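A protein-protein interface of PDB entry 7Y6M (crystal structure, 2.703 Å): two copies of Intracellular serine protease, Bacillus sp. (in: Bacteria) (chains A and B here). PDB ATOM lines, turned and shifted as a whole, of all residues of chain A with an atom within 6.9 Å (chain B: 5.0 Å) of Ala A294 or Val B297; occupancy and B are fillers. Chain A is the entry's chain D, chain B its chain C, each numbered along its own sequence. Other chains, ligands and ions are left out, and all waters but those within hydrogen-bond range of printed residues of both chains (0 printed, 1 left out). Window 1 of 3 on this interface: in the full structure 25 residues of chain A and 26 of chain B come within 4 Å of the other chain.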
ATOM      1  N   THR A 288      -1.239   6.300  12.466  1.00  0.00           N
ATOM      2  CA  THR A 288      -2.583   6.726  12.114  1.00  0.00           C
ATOM      3  C   THR A 288      -2.694   6.928  10.606  1.00  0.00           C
ATOM      4  O   THR A 288      -1.698   6.938   9.867  1.00  0.00           O
ATOM      5  CB  THR A 288      -2.974   8.021  12.841  1.00  0.00           C
ATOM      6  OG1 THR A 288      -2.516   9.145  12.091  1.00  0.00           O
ATOM      7  CG2 THR A 288      -2.339   8.084  14.166  1.00  0.00           C
ATOM      8  N   GLU A 289      -3.946   7.096  10.163  1.00  0.00           N
ATOM      9  CA  GLU A 289      -4.226   7.294   8.744  1.00  0.00           C
ATOM     10  C   GLU A 289      -3.559   8.538   8.160  1.00  0.00           C
ATOM     11  O   GLU A 289      -3.071   8.462   7.018  1.00  0.00           O
ATOM     12  CB  GLU A 289      -5.745   7.321   8.539  1.00  0.00           C
ATOM     13  CG  GLU A 289      -6.166   7.134   7.113  1.00  0.00           C
ATOM     14  CD  GLU A 289      -6.286   8.449   6.399  1.00  0.00           C
ATOM     15  OE1 GLU A 289      -6.231   9.493   7.095  1.00  0.00           O
ATOM     16  OE2 GLU A 289      -6.439   8.438   5.153  1.00  0.00           O
ATOM     17  N   PRO A 290      -3.500   9.686   8.847  1.00  0.00           N
ATOM     18  CA  PRO A 290      -2.718  10.803   8.293  1.00  0.00           C
ATOM     19  C   PRO A 290      -1.214  10.555   8.299  1.00  0.00           C
ATOM     20  O   PRO A 290      -0.508  11.022   7.385  1.00  0.00           O
ATOM     21  CB  PRO A 290      -3.109  11.980   9.196  1.00  0.00           C
ATOM     22  CG  PRO A 290      -4.463  11.624   9.684  1.00  0.00           C
ATOM     23  CD  PRO A 290      -4.395  10.144   9.920  1.00  0.00           C
ATOM     24  N   GLU A 291      -0.700   9.819   9.292  1.00  0.00           N
ATOM     25  CA  GLU A 291       0.726   9.504   9.285  1.00  0.00           C
ATOM     26  C   GLU A 291       1.077   8.563   8.143  1.00  0.00           C
ATOM     27  O   GLU A 291       2.101   8.751   7.474  1.00  0.00           O
ATOM     28  CB  GLU A 291       1.155   8.872  10.601  1.00  0.00           C
ATOM     29  CG  GLU A 291       1.044   9.728  11.800  1.00  0.00           C
ATOM     30  CD  GLU A 291       1.338   8.907  13.018  1.00  0.00           C
ATOM     31  OE1 GLU A 291       2.274   9.261  13.771  1.00  0.00           O
ATOM     32  OE2 GLU A 291       0.663   7.866  13.202  1.00  0.00           O
ATOM     33  N   ILE A 292       0.264   7.525   7.930  1.00  0.00           N
ATOM     34  CA  ILE A 292       0.569   6.592   6.850  1.00  0.00           C
ATOM     35  C   ILE A 292       0.514   7.312   5.514  1.00  0.00           C
ATOM     36  O   ILE A 292       1.378   7.121   4.652  1.00  0.00           O
ATOM     37  CB  ILE A 292      -0.391   5.393   6.880  1.00  0.00           C
ATOM     38  CG1 ILE A 292      -0.066   4.507   8.065  1.00  0.00           C
ATOM     39  CG2 ILE A 292      -0.253   4.565   5.607  1.00  0.00           C
ATOM     40  CD1 ILE A 292       1.301   3.844   7.941  1.00  0.00           C
ATOM     41  N   TYR A 293      -0.503   8.161   5.326  1.00  0.00           N
ATOM     42  CA  TYR A 293      -0.563   8.967   4.115  1.00  0.00           C
ATOM     43  C   TYR A 293       0.719   9.758   3.919  1.00  0.00           C
ATOM     44  O   TYR A 293       1.323   9.709   2.841  1.00  0.00           O
ATOM     45  CB  TYR A 293      -1.747   9.928   4.133  1.00  0.00           C
ATOM     46  CG  TYR A 293      -1.788  10.697   2.839  1.00  0.00           C
ATOM     47  CD1 TYR A 293      -2.257  10.101   1.698  1.00  0.00           C
ATOM     48  CD2 TYR A 293      -1.303  11.993   2.745  1.00  0.00           C
ATOM     49  CE1 TYR A 293      -2.290  10.772   0.504  1.00  0.00           C
ATOM     50  CE2 TYR A 293      -1.328  12.678   1.540  1.00  0.00           C
ATOM     51  CZ  TYR A 293      -1.829  12.049   0.425  1.00  0.00           C
ATOM     52  OH  TYR A 293      -1.884  12.669  -0.796  1.00  0.00           O
ATOM     53  N   ALA A 294       1.136  10.518   4.946  1.00  0.00           N
ATOM     54  CA  ALA A 294       2.429  11.202   4.870  1.00  0.00           C
ATOM     55  C   ALA A 294       3.530  10.239   4.425  1.00  0.00           C
ATOM     56  O   ALA A 294       4.338  10.559   3.538  1.00  0.00           O
ATOM     57  CB  ALA A 294       2.783  11.836   6.216  1.00  0.00           C
ATOM     58  N   GLN A 295       3.549   9.037   4.997  1.00  0.00           N
ATOM     59  CA  GLN A 295       4.573   8.079   4.615  1.00  0.00           C
ATOM     60  C   GLN A 295       4.338   7.523   3.220  1.00  0.00           C
ATOM     61  O   GLN A 295       5.279   7.004   2.612  1.00  0.00           O
ATOM     62  CB  GLN A 295       4.643   6.956   5.650  1.00  0.00           C
ATOM     63  CG  GLN A 295       4.944   7.475   7.037  1.00  0.00           C
ATOM     64  CD  GLN A 295       6.366   7.890   7.138  1.00  0.00           C
ATOM     65  OE1 GLN A 295       7.209   7.357   6.433  1.00  0.00           O
ATOM     66  NE2 GLN A 295       6.653   8.836   8.003  1.00  0.00           N
ATOM     67  N   LEU A 296       3.115   7.613   2.693  1.00  0.00           N
ATOM     68  CA  LEU A 296       2.941   7.330   1.275  1.00  0.00           C
ATOM     69  C   LEU A 296       3.664   8.370   0.437  1.00  0.00           C
ATOM     70  O   LEU A 296       4.492   8.041  -0.423  1.00  0.00           O
ATOM     71  CB  LEU A 296       1.464   7.302   0.911  1.00  0.00           C
ATOM     72  CG  LEU A 296       1.176   6.972  -0.552  1.00  0.00           C
ATOM     73  CD1 LEU A 296       1.881   5.693  -0.990  1.00  0.00           C
ATOM     74  CD2 LEU A 296      -0.318   6.838  -0.745  1.00  0.00           C
ATOM     75  N   VAL A 297       3.380   9.643   0.702  1.00  0.00           N
ATOM     76  CA  VAL A 297       3.908  10.711  -0.126  1.00  0.00           C
ATOM     77  C   VAL A 297       5.417  10.823   0.016  1.00  0.00           C
ATOM     78  O   VAL A 297       6.091  11.330  -0.891  1.00  0.00           O
ATOM     79  CB  VAL A 297       3.175  12.014   0.230  1.00  0.00           C
ATOM     80  CG1 VAL A 297       3.955  13.219  -0.261  1.00  0.00           C
ATOM     81  CG2 VAL A 297       1.764  11.974  -0.361  1.00  0.00           C
ATOM     82  N   ARG A 298       5.975  10.333   1.126  1.00  0.00           N
ATOM     83  CA  ARG A 298       7.421  10.399   1.286  1.00  0.00           C
ATOM     84  C   ARG A 298       8.106   9.429   0.340  1.00  0.00           C
ATOM     85  O   ARG A 298       9.173   9.733  -0.210  1.00  0.00           O
ATOM     86  CB  ARG A 298       7.820  10.114   2.730  1.00  0.00           C
ATOM     87  CG  ARG A 298       9.317  10.167   2.920  1.00  0.00           C
ATOM     88  CD  ARG A 298       9.702  10.140   4.361  1.00  0.00           C
ATOM     89  NE  ARG A 298      10.981  10.810   4.537  1.00  0.00           N
ATOM     90  CZ  ARG A 298      11.771  10.629   5.589  1.00  0.00           C
ATOM     91  NH1 ARG A 298      11.402   9.793   6.562  1.00  0.00           N
ATOM     92  NH2 ARG A 298      12.925  11.286   5.666  1.00  0.00           N
ATOM     93  N   ARG A 299       7.488   8.259   0.154  1.00  0.00           N
ATOM     94  CA  ARG A 299       8.038   7.208  -0.745  1.00  0.00           C
ATOM     95  C   ARG A 299       7.659   7.534  -2.194  1.00  0.00           C
ATOM     96  O   ARG A 299       7.649   6.605  -3.026  1.00  0.00           O
ATOM     97  CB  ARG A 299       7.513   5.828  -0.334  1.00  0.00           C
ATOM     98  CG  ARG A 299       7.703   5.506   1.140  1.00  0.00           C
ATOM     99  CD  ARG A 299       7.564   4.023   1.432  1.00  0.00           C
ATOM    100  NE  ARG A 299       8.833   3.407   1.791  1.00  0.00           N
ATOM    101  CZ  ARG A 299       9.430   3.546   2.969  1.00  0.00           C
ATOM    102  NH1 ARG A 299       8.870   4.286   3.911  1.00  0.00           N
ATOM    103  NH2 ARG A 299      10.583   2.946   3.203  1.00  0.00           N
ATOM    104  N   TYR B 293       0.916  18.278   6.163  1.00  0.00           N
ATOM    105  CA  TYR B 293       1.774  17.458   7.027  1.00  0.00           C
ATOM    106  C   TYR B 293       2.594  16.471   6.200  1.00  0.00           C
ATOM    107  O   TYR B 293       3.824  16.400   6.333  1.00  0.00           O
ATOM    108  CB  TYR B 293       0.938  16.721   8.089  1.00  0.00           C
ATOM    109  CG  TYR B 293       1.752  15.739   8.923  1.00  0.00           C
ATOM    110  CD1 TYR B 293       2.731  16.188   9.811  1.00  0.00           C
ATOM    111  CD2 TYR B 293       1.563  14.365   8.811  1.00  0.00           C
ATOM    112  CE1 TYR B 293       3.493  15.301  10.569  1.00  0.00           C
ATOM    113  CE2 TYR B 293       2.317  13.472   9.568  1.00  0.00           C
ATOM    114  CZ  TYR B 293       3.284  13.953  10.439  1.00  0.00           C
ATOM    115  OH  TYR B 293       4.041  13.078  11.194  1.00  0.00           O
ATOM    116  N   ALA B 294       1.922  15.713   5.326  1.00  0.00           N
ATOM    117  CA  ALA B 294       2.613  14.909   4.320  1.00  0.00           C
ATOM    118  C   ALA B 294       3.692  15.717   3.606  1.00  0.00           C
ATOM    119  O   ALA B 294       4.850  15.294   3.497  1.00  0.00           O
ATOM    120  CB  ALA B 294       1.598  14.380   3.311  1.00  0.00           C
ATOM    121  N   GLN B 295       3.313  16.884   3.099  1.00  0.00           N
ATOM    122  CA  GLN B 295       4.272  17.749   2.441  1.00  0.00           C
ATOM    123  C   GLN B 295       5.391  18.147   3.386  1.00  0.00           C
ATOM    124  O   GLN B 295       6.540  18.313   2.952  1.00  0.00           O
ATOM    125  CB  GLN B 295       3.555  18.982   1.892  1.00  0.00           C
ATOM    126  CG  GLN B 295       2.641  18.679   0.715  1.00  0.00           C
ATOM    127  CD  GLN B 295       3.399  18.024  -0.412  1.00  0.00           C
ATOM    128  OE1 GLN B 295       4.570  18.353  -0.650  1.00  0.00           O
ATOM    129  NE2 GLN B 295       2.759  17.060  -1.091  1.00  0.00           N
ATOM    130  N   LEU B 296       5.089  18.291   4.681  1.00  0.00           N
ATOM    131  CA  LEU B 296       6.141  18.657   5.623  1.00  0.00           C
ATOM    132  C   LEU B 296       7.130  17.512   5.796  1.00  0.00           C
ATOM    133  O   LEU B 296       8.348  17.712   5.683  1.00  0.00           O
ATOM    134  CB  LEU B 296       5.548  19.067   6.968  1.00  0.00           C
ATOM    135  CG  LEU B 296       6.587  19.434   8.034  1.00  0.00           C
ATOM    136  CD1 LEU B 296       7.056  20.853   7.833  1.00  0.00           C
ATOM    137  CD2 LEU B 296       6.026  19.261   9.447  1.00  0.00           C
ATOM    138  N   VAL B 297       6.630  16.293   6.043  1.00  0.00           N
ATOM    139  CA  VAL B 297       7.563  15.183   6.223  1.00  0.00           C
ATOM    140  C   VAL B 297       8.150  14.717   4.907  1.00  0.00           C
ATOM    141  O   VAL B 297       9.114  13.934   4.910  1.00  0.00           O
ATOM    142  CB  VAL B 297       6.942  13.974   6.938  1.00  0.00           C
ATOM    143  CG1 VAL B 297       6.098  14.434   8.116  1.00  0.00           C
ATOM    144  CG2 VAL B 297       6.145  13.153   5.972  1.00  0.00           C
ATOM    145  N   ARG B 298       7.593  15.177   3.782  1.00  0.00           N
ATOM    146  CA  ARG B 298       8.258  14.996   2.502  1.00  0.00           C
ATOM    147  C   ARG B 298       9.455  15.914   2.357  1.00  0.00           C
ATOM    148  O   ARG B 298      10.369  15.607   1.588  1.00  0.00           O
ATOM    149  CB  ARG B 298       7.277  15.238   1.366  1.00  0.00           C
ATOM    150  CG  ARG B 298       7.930  15.281   0.008  1.00  0.00           C
ATOM    151  CD  ARG B 298       6.919  15.393  -1.097  1.00  0.00           C
ATOM    152  NE  ARG B 298       7.244  14.453  -2.163  1.00  0.00           N
ATOM    153  CZ  ARG B 298       7.113  14.734  -3.449  1.00  0.00           C
ATOM    154  NH1 ARG B 298       6.668  15.938  -3.811  1.00  0.00           N
ATOM    155  NH2 ARG B 298       7.434  13.819  -4.362  1.00  0.00           N
ATOM    156  N   ARG B 299       9.487  17.014   3.097  1.00  0.00           N
ATOM    157  CA  ARG B 299      10.641  17.912   3.073  1.00  0.00           C
ATOM    158  C   ARG B 299      11.524  17.689   4.306  1.00  0.00           C
ATOM    159  O   ARG B 299      11.735  18.569   5.158  1.00  0.00           O
ATOM    160  CB  ARG B 299      10.175  19.360   2.956  1.00  0.00           C
ATOM    161  CG  ARG B 299       9.824  19.736   1.530  1.00  0.00           C
ATOM    162  CD  ARG B 299       9.090  21.050   1.479  1.00  0.00           C
ATOM    163  NE  ARG B 299       8.748  21.435   0.112  1.00  0.00           N
ATOM    164  CZ  ARG B 299       7.773  20.876  -0.596  1.00  0.00           C
ATOM    165  NH1 ARG B 299       7.027  19.887  -0.077  1.00  0.00           N
ATOM    166  NH2 ARG B 299       7.550  21.306  -1.831  1.00  0.00           N
ATOM    167  N   THR B 300      12.077  16.478   4.365  1.00  0.00           N
ATOM    168  CA  THR B 300      12.794  16.005   5.544  1.00  0.00           C
ATOM    169  C   THR B 300      13.841  14.980   5.125  1.00  0.00           C
ATOM    170  O   THR B 300      13.500  13.945   4.537  1.00  0.00           O
ATOM    171  CB  THR B 300      11.806  15.398   6.549  1.00  0.00           C
ATOM    172  OG1 THR B 300      10.980  16.439   7.083  1.00  0.00           O
ATOM    173  CG2 THR B 300      12.527  14.711   7.676  1.00  0.00           C
ATOM    174  N   ASN B 312      11.005  11.945  11.814  1.00  0.00           N
ATOM    175  CA  ASN B 312      11.224  11.614  10.417  1.00  0.00           C
ATOM    176  C   ASN B 312      12.607  12.031   9.954  1.00  0.00           C
ATOM    177  O   ASN B 312      13.154  11.436   9.023  1.00  0.00           O
ATOM    178  CB  ASN B 312      10.166  12.280   9.554  1.00  0.00           C
ATOM    179  CG  ASN B 312       8.871  11.502   9.512  1.00  0.00           C
ATOM    180  OD1 ASN B 312       8.752  10.521   8.786  1.00  0.00           O
ATOM    181  ND2 ASN B 312       7.884  11.958  10.263  1.00  0.00           N
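The backbone carbonyl oxygen (O) of Asn B312 is in hydrogen-bond range of the guanidinium group (NH2) of Arg A298, 3.4 Å away.
O of Thr B300 lies within hydrogen-bond range of NH2 of Arg A298 (2.9 Å).
The side-chain amide oxygen (OD1) of Asn B312 sits at hydrogen-bond distance from the side-chain amide nitrogen (NE2) of Gln A295 (2.8 Å).
Tyr A293 touches Ala B294, and with the chains exchanged Ala A294 touches Tyr B293.
Ala A294 touches its own counterpart, Ala B294.
Ala A294 touches Val B297, but with the chains exchanged Val A297 does not touch Ala B294 (4.2 Å).
Val A297 touches Arg B298, and with the chains exchanged Arg A298 touches Val B297.
Of the 9 pairs that touch across the chains among the printed residues, 5 have their exchanged pair printed and touching as well.
Of the 12 printed residues of chain A, 5 touch a printed residue of chain B.
Hydrophobic or aromatic side chains of chain A within 4 Å of the printed part of chain B: Tyr A293, Ala A294 and Val A297.
Among the printed residues, no Asp or Glu carboxylate lies within 4 Å of a Lys or Arg side-chain nitrogen of the other chain.
Ala A294 touches just these residues of chain B: Tyr B293, Ala B294 and Val B297.
Of the printed residues of chain B, Val A297 touches Arg B298.
Arg A299 touches none of the printed residues of chain B.
Printed residues of chain A within 4 Å of Tyr B293: Ala A294.
Of chain A, only Ala A294 and Arg A298 come within 4 Å of Val B297.
Of the printed residues of chain A, Asn B312 touches Gln A295 (2.8 Å) and Arg A298 (3.4 Å).
The nearest printed residue of chain B that does not touch Ala A294 is Arg B298 (5.7 Å).
Tyr A293 touches Ala B294 (CD2 to CB, 3.8 Å).
CB of Ala A294 touches CE2 of Tyr B293 (3.8 Å).
CA of Ala B294 touches CB of Ala A294, at 3.6 Å.
Ala A294 touches Val B297.
O of Val A297 touches NE of Arg B298, at 3.6 Å.
Val B297 touches Arg A298 (O to NE, 3.7 Å).
The backbone carbonyl oxygen (O) of Leu B296 lies within hydrogen-bond range of the side-chain hydroxyl (OG1) of Thr B300, at 3.2 Å.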
